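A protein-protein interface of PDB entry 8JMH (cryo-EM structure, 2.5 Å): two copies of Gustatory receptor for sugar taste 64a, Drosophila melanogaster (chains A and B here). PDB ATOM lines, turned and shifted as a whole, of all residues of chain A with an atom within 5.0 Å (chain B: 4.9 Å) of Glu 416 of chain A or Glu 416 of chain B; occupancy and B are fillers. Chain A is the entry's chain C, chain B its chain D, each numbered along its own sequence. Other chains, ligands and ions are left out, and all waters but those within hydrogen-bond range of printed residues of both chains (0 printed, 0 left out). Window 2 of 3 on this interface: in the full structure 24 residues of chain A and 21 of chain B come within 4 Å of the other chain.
Of the 10 printed residues of chain A, 4 touch a printed residue of chain B.
Printed residues of chain A that touch a printed residue of chain B: Trp 411, Glu 416, Ile 419 and Phe 420.
Hydrophobic or aromatic side chains of chain B within 4 Å of the printed part of chain A: Val 413 and Phe 420.
Among the printed residues, 5 pairs touch across the chains.
Among the printed residues, no Asp or Glu carboxylate lies within 4 Å of a Lys or Arg side-chain nitrogen of the other chain.
Trp 411 of chain A touches Val 413 of chain B, but with the chains exchanged Val 413 of chain A does not touch Trp 411 of chain B (13.2 Å).
Trp 411 of chain A touches Arg 417 of chain B, but with the chains exchanged Arg 417 of chain A does not touch Trp 411 of chain B (14.5 Å).
Glu 416 of chain A touches its own counterpart, Glu 416 of chain B.
Phe 420 of chain A touches its own counterpart, Phe 420 of chain B.
Positions printed for both chains: 411, 412, 413, 414, 415, 416, 417, 418, 419 and 420.
Of the 5 pairs that touch across the chains among the printed residues, 2 have their exchanged pair printed and touching as well.
Glu 416 of chain A touches just one residue of chain B: Glu 416 (3.6 Å).
Of chain A, only Glu 416 (3.6 Å) comes within 4 Å of Glu 416 of chain B.
Of the printed residues of chain B, Trp 411 of chain A touches Val 413 and Arg 417.
Of the printed residues of chain A, Arg 417 of chain B touches Trp 411 (3.2 Å).
Trp 411 of chain B touches none of the printed residues of chain A.
The nearest printed residue of chain B that does not touch Glu 416 of chain A is Phe 420 of chain B (6.2 Å).
The nearest printed residue of chain A that does not touch Glu 416 of chain B is Trp 411 of chain A (6.3 Å).
The nearest printed residue of chain A that does not touch Val 413 of chain B is Glu 416 of chain A (6.6 Å).
Among the printed residues, pairs that only touch across the chains: Trp 411 of chain A with Val 413 of chain B (3.4 Å), Trp 411 of chain A with Arg 417 of chain B (3.2 Å), Glu 416 of chain A with Glu 416 of chain B (3.6 Å), Ile 419 of chain A with Phe 420 of chain B (3.7 Å) and Phe 420 of chain A with Phe 420 of chain B (3.6 Å).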
ATOM      1  N   TRP A 411       2.240  18.845   0.120  1.00  0.00           N
ATOM      2  CA  TRP A 411       1.619  17.936   1.072  1.00  0.00           C
ATOM      3  C   TRP A 411       2.653  16.980   1.652  1.00  0.00           C
ATOM      4  O   TRP A 411       3.500  16.441   0.935  1.00  0.00           O
ATOM      5  CB  TRP A 411       0.501  17.148   0.392  1.00  0.00           C
ATOM      6  CG  TRP A 411      -0.252  16.251   1.322  1.00  0.00           C
ATOM      7  CD1 TRP A 411      -0.090  14.906   1.470  1.00  0.00           C
ATOM      8  CD2 TRP A 411      -1.290  16.632   2.229  1.00  0.00           C
ATOM      9  NE1 TRP A 411      -0.962  14.426   2.415  1.00  0.00           N
ATOM     10  CE2 TRP A 411      -1.710  15.467   2.897  1.00  0.00           C
ATOM     11  CE3 TRP A 411      -1.905  17.847   2.544  1.00  0.00           C
ATOM     12  CZ2 TRP A 411      -2.714  15.479   3.858  1.00  0.00           C
ATOM     13  CZ3 TRP A 411      -2.902  17.856   3.498  1.00  0.00           C
ATOM     14  CH2 TRP A 411      -3.297  16.680   4.144  1.00  0.00           C
ATOM     15  N   CYS A 412       2.576  16.771   2.963  1.00  0.00           N
ATOM     16  CA  CYS A 412       3.488  15.876   3.658  1.00  0.00           C
ATOM     17  C   CYS A 412       2.784  15.337   4.896  1.00  0.00           C
ATOM     18  O   CYS A 412       1.619  15.646   5.159  1.00  0.00           O
ATOM     19  CB  CYS A 412       4.793  16.590   4.021  1.00  0.00           C
ATOM     20  SG  CYS A 412       4.578  18.068   5.033  1.00  0.00           S
ATOM     21  N   VAL A 413       3.508  14.520   5.662  1.00  0.00           N
ATOM     22  CA  VAL A 413       2.932  13.929   6.864  1.00  0.00           C
ATOM     23  C   VAL A 413       2.605  15.003   7.891  1.00  0.00           C
ATOM     24  O   VAL A 413       1.607  14.896   8.615  1.00  0.00           O
ATOM     25  CB  VAL A 413       3.889  12.872   7.445  1.00  0.00           C
ATOM     26  CG1 VAL A 413       3.435  12.449   8.829  1.00  0.00           C
ATOM     27  CG2 VAL A 413       3.977  11.672   6.517  1.00  0.00           C
ATOM     28  N   GLU A 414       3.429  16.048   7.982  1.00  0.00           N
ATOM     29  CA  GLU A 414       3.200  17.085   8.983  1.00  0.00           C
ATOM     30  C   GLU A 414       1.877  17.803   8.747  1.00  0.00           C
ATOM     31  O   GLU A 414       1.144  18.087   9.701  1.00  0.00           O
ATOM     32  CB  GLU A 414       4.359  18.077   8.978  1.00  0.00           C
ATOM     33  CG  GLU A 414       5.670  17.467   9.430  1.00  0.00           C
ATOM     34  CD  GLU A 414       5.684  17.154  10.913  1.00  0.00           C
ATOM     35  OE1 GLU A 414       5.039  17.893  11.685  1.00  0.00           O
ATOM     36  OE2 GLU A 414       6.338  16.166  11.306  1.00  0.00           O
ATOM     37  N   VAL A 415       1.556  18.110   7.490  1.00  0.00           N
ATOM     38  CA  VAL A 415       0.261  18.713   7.195  1.00  0.00           C
ATOM     39  C   VAL A 415      -0.860  17.743   7.537  1.00  0.00           C
ATOM     40  O   VAL A 415      -1.892  18.135   8.096  1.00  0.00           O
ATOM     41  CB  VAL A 415       0.191  19.156   5.723  1.00  0.00           C
ATOM     42  CG1 VAL A 415      -1.087  19.936   5.469  1.00  0.00           C
ATOM     43  CG2 VAL A 415       1.393  19.997   5.363  1.00  0.00           C
ATOM     44  N   GLU A 416      -0.681  16.464   7.207  1.00  0.00           N
ATOM     45  CA  GLU A 416      -1.689  15.466   7.543  1.00  0.00           C
ATOM     46  C   GLU A 416      -1.881  15.378   9.051  1.00  0.00           C
ATOM     47  O   GLU A 416      -3.012  15.290   9.541  1.00  0.00           O
ATOM     48  CB  GLU A 416      -1.288  14.109   6.966  1.00  0.00           C
ATOM     49  CG  GLU A 416      -2.448  13.150   6.785  1.00  0.00           C
ATOM     50  CD  GLU A 416      -1.998  11.764   6.379  1.00  0.00           C
ATOM     51  OE1 GLU A 416      -0.779  11.564   6.193  1.00  0.00           O
ATOM     52  OE2 GLU A 416      -2.861  10.872   6.245  1.00  0.00           O
ATOM     53  N   ARG A 417      -0.781  15.396   9.807  1.00  0.00           N
ATOM     54  CA  ARG A 417      -0.889  15.410  11.262  1.00  0.00           C
ATOM     55  C   ARG A 417      -1.620  16.656  11.740  1.00  0.00           C
ATOM     56  O   ARG A 417      -2.528  16.577  12.574  1.00  0.00           O
ATOM     57  CB  ARG A 417       0.500  15.344  11.894  1.00  0.00           C
ATOM     58  CG  ARG A 417       1.198  14.010  11.770  1.00  0.00           C
ATOM     59  CD  ARG A 417       2.532  14.048  12.489  1.00  0.00           C
ATOM     60  NE  ARG A 417       2.365  14.195  13.930  1.00  0.00           N
ATOM     61  CZ  ARG A 417       3.356  14.176  14.809  1.00  0.00           C
ATOM     62  NH1 ARG A 417       4.614  14.020  14.430  1.00  0.00           N
ATOM     63  NH2 ARG A 417       3.079  14.314  16.102  1.00  0.00           N
ATOM     64  N   LEU A 418      -1.232  17.822  11.219  1.00  0.00           N
ATOM     65  CA  LEU A 418      -1.840  19.068  11.668  1.00  0.00           C
ATOM     66  C   LEU A 418      -3.324  19.112  11.333  1.00  0.00           C
ATOM     67  O   LEU A 418      -4.148  19.471  12.181  1.00  0.00           O
ATOM     68  CB  LEU A 418      -1.110  20.255  11.041  1.00  0.00           C
ATOM     69  CG  LEU A 418      -1.518  21.648  11.525  1.00  0.00           C
ATOM     70  CD1 LEU A 418      -1.462  21.749  13.040  1.00  0.00           C
ATOM     71  CD2 LEU A 418      -0.633  22.701  10.884  1.00  0.00           C
ATOM     72  N   ILE A 419      -3.689  18.735  10.107  1.00  0.00           N
ATOM     73  CA  ILE A 419      -5.091  18.790   9.704  1.00  0.00           C
ATOM     74  C   ILE A 419      -5.927  17.850  10.561  1.00  0.00           C
ATOM     75  O   ILE A 419      -7.061  18.170  10.934  1.00  0.00           O
ATOM     76  CB  ILE A 419      -5.228  18.471   8.204  1.00  0.00           C
ATOM     77  CG1 ILE A 419      -4.843  19.698   7.377  1.00  0.00           C
ATOM     78  CG2 ILE A 419      -6.649  18.021   7.879  1.00  0.00           C
ATOM     79  CD1 ILE A 419      -4.832  19.459   5.888  1.00  0.00           C
ATOM     80  N   PHE A 420      -5.388  16.673  10.879  1.00  0.00           N
ATOM     81  CA  PHE A 420      -6.124  15.738  11.723  1.00  0.00           C
ATOM     82  C   PHE A 420      -6.362  16.321  13.109  1.00  0.00           C
ATOM     83  O   PHE A 420      -7.447  16.162  13.679  1.00  0.00           O
ATOM     84  CB  PHE A 420      -5.372  14.412  11.819  1.00  0.00           C
ATOM     85  CG  PHE A 420      -6.158  13.318  12.482  1.00  0.00           C
ATOM     86  CD1 PHE A 420      -7.147  12.644  11.791  1.00  0.00           C
ATOM     87  CD2 PHE A 420      -5.909  12.968  13.796  1.00  0.00           C
ATOM     88  CE1 PHE A 420      -7.872  11.640  12.398  1.00  0.00           C
ATOM     89  CE2 PHE A 420      -6.631  11.965  14.407  1.00  0.00           C
ATOM     90  CZ  PHE A 420      -7.613  11.300  13.707  1.00  0.00           C
ATOM     91  N   TRP B 411      -6.374   4.361  -5.887  1.00  0.00           N
ATOM     92  CA  TRP B 411      -6.236   5.043  -4.609  1.00  0.00           C
ATOM     93  C   TRP B 411      -4.903   5.773  -4.531  1.00  0.00           C
ATOM     94  O   TRP B 411      -3.856   5.234  -4.902  1.00  0.00           O
ATOM     95  CB  TRP B 411      -6.349   4.038  -3.463  1.00  0.00           C
ATOM     96  CG  TRP B 411      -6.313   4.666  -2.107  1.00  0.00           C
ATOM     97  CD1 TRP B 411      -5.244   4.734  -1.266  1.00  0.00           C
ATOM     98  CD2 TRP B 411      -7.397   5.310  -1.431  1.00  0.00           C
ATOM     99  NE1 TRP B 411      -5.593   5.382  -0.109  1.00  0.00           N
ATOM    100  CE2 TRP B 411      -6.911   5.746  -0.184  1.00  0.00           C
ATOM    101  CE3 TRP B 411      -8.732   5.562  -1.758  1.00  0.00           C
ATOM    102  CZ2 TRP B 411      -7.710   6.418   0.734  1.00  0.00           C
ATOM    103  CZ3 TRP B 411      -9.523   6.228  -0.844  1.00  0.00           C
ATOM    104  CH2 TRP B 411      -9.010   6.648   0.386  1.00  0.00           C
ATOM    105  N   CYS B 412      -4.946   7.010  -4.044  1.00  0.00           N
ATOM    106  CA  CYS B 412      -3.749   7.824  -3.896  1.00  0.00           C
ATOM    107  C   CYS B 412      -3.961   8.792  -2.741  1.00  0.00           C
ATOM    108  O   CYS B 412      -4.999   8.780  -2.075  1.00  0.00           O
ATOM    109  CB  CYS B 412      -3.421   8.564  -5.196  1.00  0.00           C
ATOM    110  SG  CYS B 412      -4.742   9.633  -5.803  1.00  0.00           S
ATOM    111  N   VAL B 413      -2.958   9.640  -2.508  1.00  0.00           N
ATOM    112  CA  VAL B 413      -3.039  10.601  -1.413  1.00  0.00           C
ATOM    113  C   VAL B 413      -4.152  11.609  -1.659  1.00  0.00           C
ATOM    114  O   VAL B 413      -4.805  12.065  -0.713  1.00  0.00           O
ATOM    115  CB  VAL B 413      -1.682  11.300  -1.221  1.00  0.00           C
ATOM    116  CG1 VAL B 413      -1.827  12.496  -0.298  1.00  0.00           C
ATOM    117  CG2 VAL B 413      -0.655  10.322  -0.677  1.00  0.00           C
ATOM    118  N   GLU B 414      -4.378  11.991  -2.916  1.00  0.00           N
ATOM    119  CA  GLU B 414      -5.407  12.982  -3.212  1.00  0.00           C
ATOM    120  C   GLU B 414      -6.794  12.467  -2.858  1.00  0.00           C
ATOM    121  O   GLU B 414      -7.617  13.210  -2.308  1.00  0.00           O
ATOM    122  CB  GLU B 414      -5.338  13.376  -4.685  1.00  0.00           C
ATOM    123  CG  GLU B 414      -4.063  14.106  -5.047  1.00  0.00           C
ATOM    124  CD  GLU B 414      -4.018  15.512  -4.482  1.00  0.00           C
ATOM    125  OE1 GLU B 414      -5.089  16.143  -4.366  1.00  0.00           O
ATOM    126  OE2 GLU B 414      -2.911  15.984  -4.150  1.00  0.00           O
ATOM    127  N   VAL B 415      -7.078  11.199  -3.163  1.00  0.00           N
ATOM    128  CA  VAL B 415      -8.369  10.630  -2.793  1.00  0.00           C
ATOM    129  C   VAL B 415      -8.512  10.592  -1.279  1.00  0.00           C
ATOM    130  O   VAL B 415      -9.594  10.845  -0.740  1.00  0.00           O
ATOM    131  CB  VAL B 415      -8.546   9.230  -3.408  1.00  0.00           C
ATOM    132  CG1 VAL B 415      -9.943   8.707  -3.126  1.00  0.00           C
ATOM    133  CG2 VAL B 415      -8.304   9.271  -4.896  1.00  0.00           C
ATOM    134  N   GLU B 416      -7.433  10.264  -0.569  1.00  0.00           N
ATOM    135  CA  GLU B 416      -7.487  10.246   0.888  1.00  0.00           C
ATOM    136  C   GLU B 416      -7.796  11.634   1.437  1.00  0.00           C
ATOM    137  O   GLU B 416      -8.639  11.789   2.328  1.00  0.00           O
ATOM    138  CB  GLU B 416      -6.164   9.724   1.447  1.00  0.00           C
ATOM    139  CG  GLU B 416      -6.268   9.155   2.848  1.00  0.00           C
ATOM    140  CD  GLU B 416      -4.921   8.755   3.413  1.00  0.00           C
ATOM    141  OE1 GLU B 416      -3.912   8.878   2.687  1.00  0.00           O
ATOM    142  OE2 GLU B 416      -4.869   8.319   4.581  1.00  0.00           O
ATOM    143  N   ARG B 417      -7.128  12.659   0.904  1.00  0.00           N
ATOM    144  CA  ARG B 417      -7.394  14.027   1.337  1.00  0.00           C
ATOM    145  C   ARG B 417      -8.842  14.408   1.072  1.00  0.00           C
ATOM    146  O   ARG B 417      -9.521  14.975   1.938  1.00  0.00           O
ATOM    147  CB  ARG B 417      -6.460  14.996   0.615  1.00  0.00           C
ATOM    148  CG  ARG B 417      -5.007  14.912   1.015  1.00  0.00           C
ATOM    149  CD  ARG B 417      -4.189  15.919   0.228  1.00  0.00           C
ATOM    150  NE  ARG B 417      -4.550  17.291   0.562  1.00  0.00           N
ATOM    151  CZ  ARG B 417      -3.948  18.368   0.075  1.00  0.00           C
ATOM    152  NH1 ARG B 417      -2.946  18.272  -0.784  1.00  0.00           N
ATOM    153  NH2 ARG B 417      -4.362  19.572   0.459  1.00  0.00           N
ATOM    154  N   LEU B 418      -9.330  14.114  -0.134  1.00  0.00           N
ATOM    155  CA  LEU B 418     -10.693  14.483  -0.489  1.00  0.00           C
ATOM    156  C   LEU B 418     -11.702  13.777   0.404  1.00  0.00           C
ATOM    157  O   LEU B 418     -12.662  14.394   0.877  1.00  0.00           O
ATOM    158  CB  LEU B 418     -10.953  14.157  -1.959  1.00  0.00           C
ATOM    159  CG  LEU B 418     -12.290  14.615  -2.541  1.00  0.00           C
ATOM    160  CD1 LEU B 418     -12.531  16.092  -2.280  1.00  0.00           C
ATOM    161  CD2 LEU B 418     -12.341  14.318  -4.029  1.00  0.00           C
ATOM    162  N   ILE B 419     -11.501  12.481   0.648  1.00  0.00           N
ATOM    163  CA  ILE B 419     -12.428  11.731   1.487  1.00  0.00           C
ATOM    164  C   ILE B 419     -12.407  12.267   2.908  1.00  0.00           C
ATOM    165  O   ILE B 419     -13.455  12.404   3.547  1.00  0.00           O
ATOM    166  CB  ILE B 419     -12.097  10.228   1.437  1.00  0.00           C
ATOM    167  CG1 ILE B 419     -12.626   9.625   0.134  1.00  0.00           C
ATOM    168  CG2 ILE B 419     -12.685   9.509   2.647  1.00  0.00           C
ATOM    169  CD1 ILE B 419     -12.260   8.178  -0.068  1.00  0.00           C
ATOM    170  N   PHE B 420     -11.220  12.578   3.430  1.00  0.00           N
ATOM    171  CA  PHE B 420     -11.143  13.140   4.774  1.00  0.00           C
ATOM    172  C   PHE B 420     -11.887  14.465   4.852  1.00  0.00           C
ATOM    173  O   PHE B 420     -12.615  14.721   5.819  1.00  0.00           O
ATOM    174  CB  PHE B 420      -9.683  13.315   5.186  1.00  0.00           C
ATOM    175  CG  PHE B 420      -9.502  13.677   6.631  1.00  0.00           C
ATOM    176  CD1 PHE B 420      -9.597  12.711   7.615  1.00  0.00           C
ATOM    177  CD2 PHE B 420      -9.237  14.981   7.006  1.00  0.00           C
ATOM    178  CE1 PHE B 420      -9.433  13.038   8.944  1.00  0.00           C
ATOM    179  CE2 PHE B 420      -9.072  15.315   8.333  1.00  0.00           C
ATOM    180  CZ  PHE B 420      -9.169  14.342   9.303  1.00  0.00           C
